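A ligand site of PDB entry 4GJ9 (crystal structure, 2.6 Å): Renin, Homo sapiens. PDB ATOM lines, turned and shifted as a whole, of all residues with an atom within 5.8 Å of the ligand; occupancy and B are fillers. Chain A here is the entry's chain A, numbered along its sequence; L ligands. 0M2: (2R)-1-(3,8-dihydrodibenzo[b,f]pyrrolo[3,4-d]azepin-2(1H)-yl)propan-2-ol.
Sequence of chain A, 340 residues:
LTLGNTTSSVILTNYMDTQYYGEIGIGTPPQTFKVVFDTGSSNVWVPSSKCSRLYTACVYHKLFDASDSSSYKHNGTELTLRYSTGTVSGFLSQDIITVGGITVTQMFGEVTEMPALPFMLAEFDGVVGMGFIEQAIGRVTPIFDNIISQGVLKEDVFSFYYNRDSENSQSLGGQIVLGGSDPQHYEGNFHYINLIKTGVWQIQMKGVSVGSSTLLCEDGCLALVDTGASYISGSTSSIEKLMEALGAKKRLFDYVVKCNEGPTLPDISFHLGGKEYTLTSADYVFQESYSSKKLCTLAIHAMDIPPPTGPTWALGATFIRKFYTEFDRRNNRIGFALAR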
ATOM      1  N   THR A  18      -1.531   9.198 -19.377  1.00  0.00           N
ATOM      2  CA  THR A  18      -1.831   8.323 -18.242  1.00  0.00           C
ATOM      3  C   THR A  18      -2.837   8.912 -17.281  1.00  0.00           C
ATOM      4  O   THR A  18      -3.480   8.148 -16.561  1.00  0.00           O
ATOM      5  CB  THR A  18      -0.534   7.890 -17.515  1.00  0.00           C
ATOM      6  OG1 THR A  18       0.116   9.049 -17.015  1.00  0.00           O
ATOM      7  CG2 THR A  18       0.435   7.098 -18.411  1.00  0.00           C
ATOM      8  N   GLN A  19      -2.978  10.238 -17.241  1.00  0.00           N
ATOM      9  CA  GLN A  19      -3.917  10.886 -16.330  1.00  0.00           C
ATOM     10  C   GLN A  19      -4.762  11.898 -17.090  1.00  0.00           C
ATOM     11  O   GLN A  19      -4.220  12.811 -17.707  1.00  0.00           O
ATOM     12  CB  GLN A  19      -3.166  11.561 -15.177  1.00  0.00           C
ATOM     13  CG  GLN A  19      -2.593  10.604 -14.129  1.00  0.00           C
ATOM     14  CD  GLN A  19      -1.756  11.323 -13.095  1.00  0.00           C
ATOM     15  OE1 GLN A  19      -2.124  12.376 -12.577  1.00  0.00           O
ATOM     16  NE2 GLN A  19      -0.601  10.755 -12.736  1.00  0.00           N
ATOM     17  N   TYR A  20      -6.066  11.723 -17.059  1.00  0.00           N
ATOM     18  CA  TYR A  20      -7.039  12.604 -17.732  1.00  0.00           C
ATOM     19  C   TYR A  20      -7.971  13.156 -16.667  1.00  0.00           C
ATOM     20  O   TYR A  20      -8.654  12.397 -16.002  1.00  0.00           O
ATOM     21  CB  TYR A  20      -7.832  11.831 -18.817  1.00  0.00           C
ATOM     22  CG  TYR A  20      -6.999  11.394 -20.005  1.00  0.00           C
ATOM     23  CD1 TYR A  20      -6.289  10.200 -19.980  1.00  0.00           C
ATOM     24  CD2 TYR A  20      -6.927  12.181 -21.151  1.00  0.00           C
ATOM     25  CE1 TYR A  20      -5.490   9.803 -21.060  1.00  0.00           C
ATOM     26  CE2 TYR A  20      -6.165  11.767 -22.249  1.00  0.00           C
ATOM     27  CZ  TYR A  20      -5.453  10.591 -22.199  1.00  0.00           C
ATOM     28  OH  TYR A  20      -4.723  10.191 -23.288  1.00  0.00           O
ATOM     29  N   TYR A  21      -7.943  14.466 -16.452  1.00  0.00           N
ATOM     30  CA  TYR A  21      -8.708  15.090 -15.369  1.00  0.00           C
ATOM     31  C   TYR A  21      -9.323  16.416 -15.766  1.00  0.00           C
ATOM     32  O   TYR A  21      -8.766  17.140 -16.594  1.00  0.00           O
ATOM     33  CB  TYR A  21      -7.851  15.224 -14.074  1.00  0.00           C
ATOM     34  CG  TYR A  21      -6.557  15.993 -14.262  1.00  0.00           C
ATOM     35  CD1 TYR A  21      -6.521  17.378 -14.187  1.00  0.00           C
ATOM     36  CD2 TYR A  21      -5.372  15.323 -14.576  1.00  0.00           C
ATOM     37  CE1 TYR A  21      -5.357  18.088 -14.438  1.00  0.00           C
ATOM     38  CE2 TYR A  21      -4.196  16.032 -14.839  1.00  0.00           C
ATOM     39  CZ  TYR A  21      -4.190  17.407 -14.751  1.00  0.00           C
ATOM     40  OH  TYR A  21      -3.014  18.100 -14.966  1.00  0.00           O
ATOM     41  N   VAL A  36     -10.556  12.945 -11.631  1.00  0.00           N
ATOM     42  CA  VAL A  36     -10.629  11.874 -12.616  1.00  0.00           C
ATOM     43  C   VAL A  36     -12.097  11.448 -12.644  1.00  0.00           C
ATOM     44  O   VAL A  36     -12.691  11.248 -11.588  1.00  0.00           O
ATOM     45  CB  VAL A  36      -9.716  10.674 -12.233  1.00  0.00           C
ATOM     46  CG1 VAL A  36      -9.984   9.467 -13.132  1.00  0.00           C
ATOM     47  CG2 VAL A  36      -8.236  11.059 -12.279  1.00  0.00           C
ATOM     48  N   ASP A  38     -14.270   8.521 -13.338  1.00  0.00           N
ATOM     49  CA  ASP A  38     -14.026   7.091 -13.315  1.00  0.00           C
ATOM     50  C   ASP A  38     -15.245   6.205 -13.406  1.00  0.00           C
ATOM     51  O   ASP A  38     -15.999   6.086 -12.450  1.00  0.00           O
ATOM     52  CB  ASP A  38     -13.144   6.763 -12.087  1.00  0.00           C
ATOM     53  CG  ASP A  38     -12.765   5.315 -11.905  1.00  0.00           C
ATOM     54  OD1 ASP A  38     -12.649   4.599 -12.917  1.00  0.00           O
ATOM     55  OD2 ASP A  38     -12.539   4.901 -10.748  1.00  0.00           O
ATOM     56  N   TRP A  45     -14.907  11.936  -4.200  1.00  0.00           N
ATOM     57  CA  TRP A  45     -13.990  12.283  -3.108  1.00  0.00           C
ATOM     58  C   TRP A  45     -12.963  13.299  -3.506  1.00  0.00           C
ATOM     59  O   TRP A  45     -12.421  13.222  -4.594  1.00  0.00           O
ATOM     60  CB  TRP A  45     -13.340  11.069  -2.432  1.00  0.00           C
ATOM     61  CG  TRP A  45     -12.318  10.348  -3.259  1.00  0.00           C
ATOM     62  CD1 TRP A  45     -12.515   9.207  -3.969  1.00  0.00           C
ATOM     63  CD2 TRP A  45     -10.921  10.672  -3.387  1.00  0.00           C
ATOM     64  NE1 TRP A  45     -11.331   8.789  -4.528  1.00  0.00           N
ATOM     65  CE2 TRP A  45     -10.340   9.676  -4.199  1.00  0.00           C
ATOM     66  CE3 TRP A  45     -10.099  11.707  -2.893  1.00  0.00           C
ATOM     67  CZ2 TRP A  45      -8.977   9.684  -4.538  1.00  0.00           C
ATOM     68  CZ3 TRP A  45      -8.765  11.740  -3.252  1.00  0.00           C
ATOM     69  CH2 TRP A  45      -8.204  10.739  -4.052  1.00  0.00           C
ATOM     70  N   TYR A  83      -8.702   1.328  -3.951  1.00  0.00           N
ATOM     71  CA  TYR A  83      -8.512   1.285  -5.386  1.00  0.00           C
ATOM     72  C   TYR A  83      -7.341   0.351  -5.736  1.00  0.00           C
ATOM     73  O   TYR A  83      -6.508   0.027  -4.872  1.00  0.00           O
ATOM     74  CB  TYR A  83      -8.271   2.703  -5.952  1.00  0.00           C
ATOM     75  CG  TYR A  83      -9.447   3.633  -5.821  1.00  0.00           C
ATOM     76  CD1 TYR A  83     -10.363   3.779  -6.856  1.00  0.00           C
ATOM     77  CD2 TYR A  83      -9.609   4.427  -4.690  1.00  0.00           C
ATOM     78  CE1 TYR A  83     -11.413   4.692  -6.771  1.00  0.00           C
ATOM     79  CE2 TYR A  83     -10.655   5.336  -4.586  1.00  0.00           C
ATOM     80  CZ  TYR A  83     -11.563   5.468  -5.636  1.00  0.00           C
ATOM     81  OH  TYR A  83     -12.611   6.360  -5.556  1.00  0.00           O
ATOM     82  N   THR A  85      -4.820   0.971  -7.261  1.00  0.00           N
ATOM     83  CA  THR A  85      -3.604   1.748  -7.173  1.00  0.00           C
ATOM     84  C   THR A  85      -3.260   2.126  -5.725  1.00  0.00           C
ATOM     85  O   THR A  85      -2.094   1.982  -5.304  1.00  0.00           O
ATOM     86  CB  THR A  85      -3.669   2.913  -8.169  1.00  0.00           C
ATOM     87  OG1 THR A  85      -5.044   3.214  -8.456  1.00  0.00           O
ATOM     88  CG2 THR A  85      -2.978   2.585  -9.475  1.00  0.00           C
ATOM     89  N   GLY A  86      -4.274   2.546  -4.966  1.00  0.00           N
ATOM     90  CA  GLY A  86      -4.130   2.941  -3.572  1.00  0.00           C
ATOM     91  C   GLY A  86      -5.434   3.050  -2.813  1.00  0.00           C
ATOM     92  O   GLY A  86      -6.498   2.799  -3.360  1.00  0.00           O
ATOM     93  N   PRO A 118       0.208   6.182  -3.798  1.00  0.00           N
ATOM     94  CA  PRO A 118       0.673   6.805  -5.048  1.00  0.00           C
ATOM     95  C   PRO A 118       0.293   8.270  -5.320  1.00  0.00           C
ATOM     96  O   PRO A 118       0.732   8.855  -6.315  1.00  0.00           O
ATOM     97  CB  PRO A 118      -0.004   5.924  -6.105  1.00  0.00           C
ATOM     98  CG  PRO A 118      -1.338   5.526  -5.453  1.00  0.00           C
ATOM     99  CD  PRO A 118      -1.152   5.632  -3.955  1.00  0.00           C
ATOM    100  N   PHE A 119      -0.526   8.856  -4.444  1.00  0.00           N
ATOM    101  CA  PHE A 119      -1.119  10.179  -4.606  1.00  0.00           C
ATOM    102  C   PHE A 119      -0.220  11.391  -4.803  1.00  0.00           C
ATOM    103  O   PHE A 119      -0.690  12.402  -5.306  1.00  0.00           O
ATOM    104  CB  PHE A 119      -2.248  10.399  -3.602  1.00  0.00           C
ATOM    105  CG  PHE A 119      -3.306   9.342  -3.801  1.00  0.00           C
ATOM    106  CD1 PHE A 119      -4.067   9.309  -4.965  1.00  0.00           C
ATOM    107  CD2 PHE A 119      -3.490   8.347  -2.859  1.00  0.00           C
ATOM    108  CE1 PHE A 119      -5.010   8.313  -5.169  1.00  0.00           C
ATOM    109  CE2 PHE A 119      -4.454   7.348  -3.060  1.00  0.00           C
ATOM    110  CZ  PHE A 119      -5.214   7.350  -4.217  1.00  0.00           C
ATOM    111  N   MET A 120       1.076  11.256  -4.538  1.00  0.00           N
ATOM    112  CA  MET A 120       2.016  12.346  -4.769  1.00  0.00           C
ATOM    113  C   MET A 120       2.275  12.473  -6.262  1.00  0.00           C
ATOM    114  O   MET A 120       2.588  13.570  -6.756  1.00  0.00           O
ATOM    115  CB  MET A 120       3.315  12.079  -4.025  1.00  0.00           C
ATOM    116  CG  MET A 120       4.093  13.321  -3.799  1.00  0.00           C
ATOM    117  SD  MET A 120       5.829  12.971  -3.545  1.00  0.00           S
ATOM    118  CE  MET A 120       5.835  12.908  -1.752  1.00  0.00           C
ATOM    119  N   LEU A 121       2.126  11.328  -6.980  1.00  0.00           N
ATOM    120  CA  LEU A 121       2.279  11.193  -8.430  1.00  0.00           C
ATOM    121  C   LEU A 121       1.039  11.705  -9.181  1.00  0.00           C
ATOM    122  O   LEU A 121       1.157  12.133 -10.332  1.00  0.00           O
ATOM    123  CB  LEU A 121       2.593   9.741  -8.799  1.00  0.00           C
ATOM    124  CG  LEU A 121       3.911   9.152  -8.224  1.00  0.00           C
ATOM    125  CD1 LEU A 121       3.955   7.638  -8.352  1.00  0.00           C
ATOM    126  CD2 LEU A 121       5.150   9.798  -8.845  1.00  0.00           C
ATOM    127  N   ALA A 122      -0.145  11.712  -8.517  1.00  0.00           N
ATOM    128  CA  ALA A 122      -1.423  12.201  -9.048  1.00  0.00           C
ATOM    129  C   ALA A 122      -1.392  13.709  -9.277  1.00  0.00           C
ATOM    130  O   ALA A 122      -1.016  14.460  -8.385  1.00  0.00           O
ATOM    131  CB  ALA A 122      -2.545  11.839  -8.113  1.00  0.00           C
ATOM    132  N   GLU A 123      -1.779  14.150 -10.483  1.00  0.00           N
ATOM    133  CA  GLU A 123      -1.853  15.550 -10.916  1.00  0.00           C
ATOM    134  C   GLU A 123      -3.207  16.134 -10.582  1.00  0.00           C
ATOM    135  O   GLU A 123      -3.406  17.358 -10.637  1.00  0.00           O
ATOM    136  CB  GLU A 123      -1.607  15.661 -12.420  1.00  0.00           C
ATOM    137  CG  GLU A 123      -0.195  15.264 -12.806  1.00  0.00           C
ATOM    138  CD  GLU A 123       0.920  16.099 -12.199  1.00  0.00           C
ATOM    139  OE1 GLU A 123       0.894  17.343 -12.363  1.00  0.00           O
ATOM    140  OE2 GLU A 123       1.809  15.504 -11.551  1.00  0.00           O
ATOM    141  N   PHE A 124      -4.134  15.237 -10.247  1.00  0.00           N
ATOM    142  CA  PHE A 124      -5.520  15.496  -9.876  1.00  0.00           C
ATOM    143  C   PHE A 124      -5.635  15.443  -8.340  1.00  0.00           C
ATOM    144  O   PHE A 124      -4.832  14.796  -7.658  1.00  0.00           O
ATOM    145  CB  PHE A 124      -6.451  14.455 -10.550  1.00  0.00           C
ATOM    146  CG  PHE A 124      -6.123  13.000 -10.257  1.00  0.00           C
ATOM    147  CD1 PHE A 124      -5.217  12.317 -11.045  1.00  0.00           C
ATOM    148  CD2 PHE A 124      -6.703  12.343  -9.191  1.00  0.00           C
ATOM    149  CE1 PHE A 124      -4.908  10.965 -10.767  1.00  0.00           C
ATOM    150  CE2 PHE A 124      -6.381  11.010  -8.911  1.00  0.00           C
ATOM    151  CZ  PHE A 124      -5.479  10.332  -9.687  1.00  0.00           C
ATOM    152  N   VAL A 127     -11.516  12.153  -7.245  1.00  0.00           N
ATOM    153  CA  VAL A 127     -12.237  11.274  -8.169  1.00  0.00           C
ATOM    154  C   VAL A 127     -13.718  11.533  -8.155  1.00  0.00           C
ATOM    155  O   VAL A 127     -14.287  11.785  -7.096  1.00  0.00           O
ATOM    156  CB  VAL A 127     -11.919   9.778  -7.842  1.00  0.00           C
ATOM    157  CG1 VAL A 127     -12.647   8.815  -8.783  1.00  0.00           C
ATOM    158  CG2 VAL A 127     -10.419   9.508  -7.861  1.00  0.00           C
ATOM    159  N   TYR A 162     -10.673  11.009 -25.212  1.00  0.00           N
ATOM    160  CA  TYR A 162      -9.302  11.108 -24.669  1.00  0.00           C
ATOM    161  C   TYR A 162      -8.380  11.362 -25.832  1.00  0.00           C
ATOM    162  O   TYR A 162      -8.330  10.551 -26.750  1.00  0.00           O
ATOM    163  CB  TYR A 162      -8.880   9.828 -23.916  1.00  0.00           C
ATOM    164  CG  TYR A 162      -9.387   9.680 -22.489  1.00  0.00           C
ATOM    165  CD1 TYR A 162     -10.081  10.715 -21.857  1.00  0.00           C
ATOM    166  CD2 TYR A 162      -9.172   8.503 -21.772  1.00  0.00           C
ATOM    167  CE1 TYR A 162     -10.558  10.568 -20.560  1.00  0.00           C
ATOM    168  CE2 TYR A 162      -9.665   8.346 -20.474  1.00  0.00           C
ATOM    169  CZ  TYR A 162     -10.341   9.387 -19.864  1.00  0.00           C
ATOM    170  OH  TYR A 162     -10.794   9.258 -18.577  1.00  0.00           O
ATOM    171  N   THR A 227     -12.730   4.306 -17.531  1.00  0.00           N
ATOM    172  CA  THR A 227     -12.197   5.629 -17.857  1.00  0.00           C
ATOM    173  C   THR A 227     -11.100   6.095 -16.904  1.00  0.00           C
ATOM    174  O   THR A 227     -10.309   6.962 -17.253  1.00  0.00           O
ATOM    175  CB  THR A 227     -13.310   6.632 -17.980  1.00  0.00           C
ATOM    176  OG1 THR A 227     -13.956   6.735 -16.722  1.00  0.00           O
ATOM    177  CG2 THR A 227     -14.318   6.243 -19.036  1.00  0.00           C
ATOM    178  N   GLY A 228     -11.083   5.508 -15.718  1.00  0.00           N
ATOM    179  CA  GLY A 228     -10.123   5.822 -14.671  1.00  0.00           C
ATOM    180  C   GLY A 228      -8.900   4.918 -14.681  1.00  0.00           C
ATOM    181  O   GLY A 228      -8.089   5.008 -13.783  1.00  0.00           O
ATOM    182  N   ALA A 229      -8.774   4.019 -15.673  1.00  0.00           N
ATOM    183  CA  ALA A 229      -7.627   3.132 -15.841  1.00  0.00           C
ATOM    184  C   ALA A 229      -6.755   3.775 -16.909  1.00  0.00           C
ATOM    185  O   ALA A 229      -7.294   4.243 -17.927  1.00  0.00           O
ATOM    186  CB  ALA A 229      -8.087   1.767 -16.285  1.00  0.00           C
ATOM    187  N   SER A 230      -5.441   3.816 -16.702  1.00  0.00           N
ATOM    188  CA  SER A 230      -4.541   4.435 -17.686  1.00  0.00           C
ATOM    189  C   SER A 230      -4.286   3.564 -18.892  1.00  0.00           C
ATOM    190  O   SER A 230      -4.073   4.051 -19.973  1.00  0.00           O
ATOM    191  CB  SER A 230      -3.200   4.816 -17.054  1.00  0.00           C
ATOM    192  OG  SER A 230      -3.393   5.768 -16.017  1.00  0.00           O
ATOM    193  N   ALA A 317      -7.579   4.130 -20.771  1.00  0.00           N
ATOM    194  CA  ALA A 317      -7.212   5.230 -21.690  1.00  0.00           C
ATOM    195  C   ALA A 317      -6.534   4.771 -22.991  1.00  0.00           C
ATOM    196  O   ALA A 317      -6.678   5.457 -24.008  1.00  0.00           O
ATOM    197  CB  ALA A 317      -6.346   6.264 -20.965  1.00  0.00           C
HETATM  198  C1  0M2 L   1      -5.920   6.988 -11.149  1.00  0.00           C
HETATM  199  C2  0M2 L   1      -4.607   7.153 -11.465  1.00  0.00           C
HETATM  200  C3  0M2 L   1      -6.579   6.738  -9.802  1.00  0.00           C
HETATM  201  C4  0M2 L   1      -6.744   7.011 -12.414  1.00  0.00           C
HETATM  202  C5  0M2 L   1      -3.454   7.342 -10.489  1.00  0.00           C
HETATM  203  C6  0M2 L   1      -4.444   7.358 -12.964  1.00  0.00           C
HETATM  204  C7  0M2 L   1      -5.842   6.319  -8.641  1.00  0.00           C
HETATM  205  C8  0M2 L   1      -7.983   6.821  -9.706  1.00  0.00           C
HETATM  206  N9  0M2 L   1      -5.840   7.586 -13.440  1.00  0.00           N
HETATM  207  C10 0M2 L   1      -3.520   6.936  -9.124  1.00  0.00           C
HETATM  208  C11 0M2 L   1      -2.394   8.192 -10.878  1.00  0.00           C
HETATM  209  N12 0M2 L   1      -4.497   6.130  -8.605  1.00  0.00           N
HETATM  210  C13 0M2 L   1      -6.523   6.002  -7.430  1.00  0.00           C
HETATM  211  C14 0M2 L   1      -8.638   6.520  -8.495  1.00  0.00           C
HETATM  212  C15 0M2 L   1      -6.160   7.302 -14.872  1.00  0.00           C
HETATM  213  C16 0M2 L   1      -2.476   7.258  -8.236  1.00  0.00           C
HETATM  214  C17 0M2 L   1      -1.360   8.530  -9.984  1.00  0.00           C
HETATM  215  C18 0M2 L   1      -7.906   6.165  -7.351  1.00  0.00           C
HETATM  216  C19 0M2 L   1      -7.311   8.112 -15.510  1.00  0.00           C
HETATM  217  C20 0M2 L   1      -1.393   8.049  -8.662  1.00  0.00           C
HETATM  218  C21 0M2 L   1      -7.110   9.616 -15.302  1.00  0.00           C
HETATM  219  O22 0M2 L   1      -7.273   7.859 -16.924  1.00  0.00           O
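OD1 of Asp 38 lies close to N of Gly 228 (3.3 Å).
The side-chain hydroxyl (OH) of Tyr 162 is in hydrogen-bond range of the backbone carbonyl oxygen (O) of Thr 227 (2.7 Å).
The side-chain hydroxyl of Ser 230 sits at hydrogen-bond distance from the backbone carbonyl oxygen of Thr 18.
OH of Tyr 83 sits at hydrogen-bond distance from NE1 of Trp 45, at 2.9 Å.
The backbone carbonyl oxygen (O) of Val 127 is in hydrogen-bond range of the backbone NH (N) of Trp 45 (3.0 Å).
The backbone carbonyl oxygen (O) of Leu 121 is in hydrogen-bond range of the side-chain amide nitrogen (NE2) of Gln 19 (3.3 Å).
The backbone NH (N) of Glu 123 sits at hydrogen-bond distance from the side-chain amide oxygen (OE1) of Gln 19, at 2.8 Å.
O of Ala 229 sits at hydrogen-bond distance from N of Ala 317.
The backbone carbonyl oxygen (O) of Gly 228 lies close to a nitrogen (N9) of the ligand, at 3.4 Å.
A nitrogen (N12) of the ligand is in hydrogen-bond range of the side-chain hydroxyl of Thr 85, at 3.0 Å.
The backbone carbonyl oxygen (O) of Thr 227 is in hydrogen-bond range of an oxygen (O22) of the ligand, 3.2 Å away.
Thr 18 touches the ligand (O to C15, 3.3 Å).
Gln 19 touches the ligand.
Tyr 20 touches the ligand.
Val 36 touches the ligand.
CG of Tyr 83 touches C18 of the ligand, at 3.3 Å.
O of Pro 118 touches C20 of the ligand (3.3 Å).
Phe 119 touches the ligand.
Ala 122 touches the ligand (N to C17, 3.7 Å).
Phe 124 touches the ligand (CZ to C1, 3.7 Å).
Val 127 touches the ligand (CG2 to C14, 3.5 Å).
Ala 229 touches the ligand.
OG of Ser 230 touches C15 of the ligand, 3.4 Å away.
Hydrophobic or aromatic side chains that line the ligand: Tyr 20, Val 36, Tyr 83, Pro 118, Phe 119, Ala 122, Phe 124 and Val 127.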
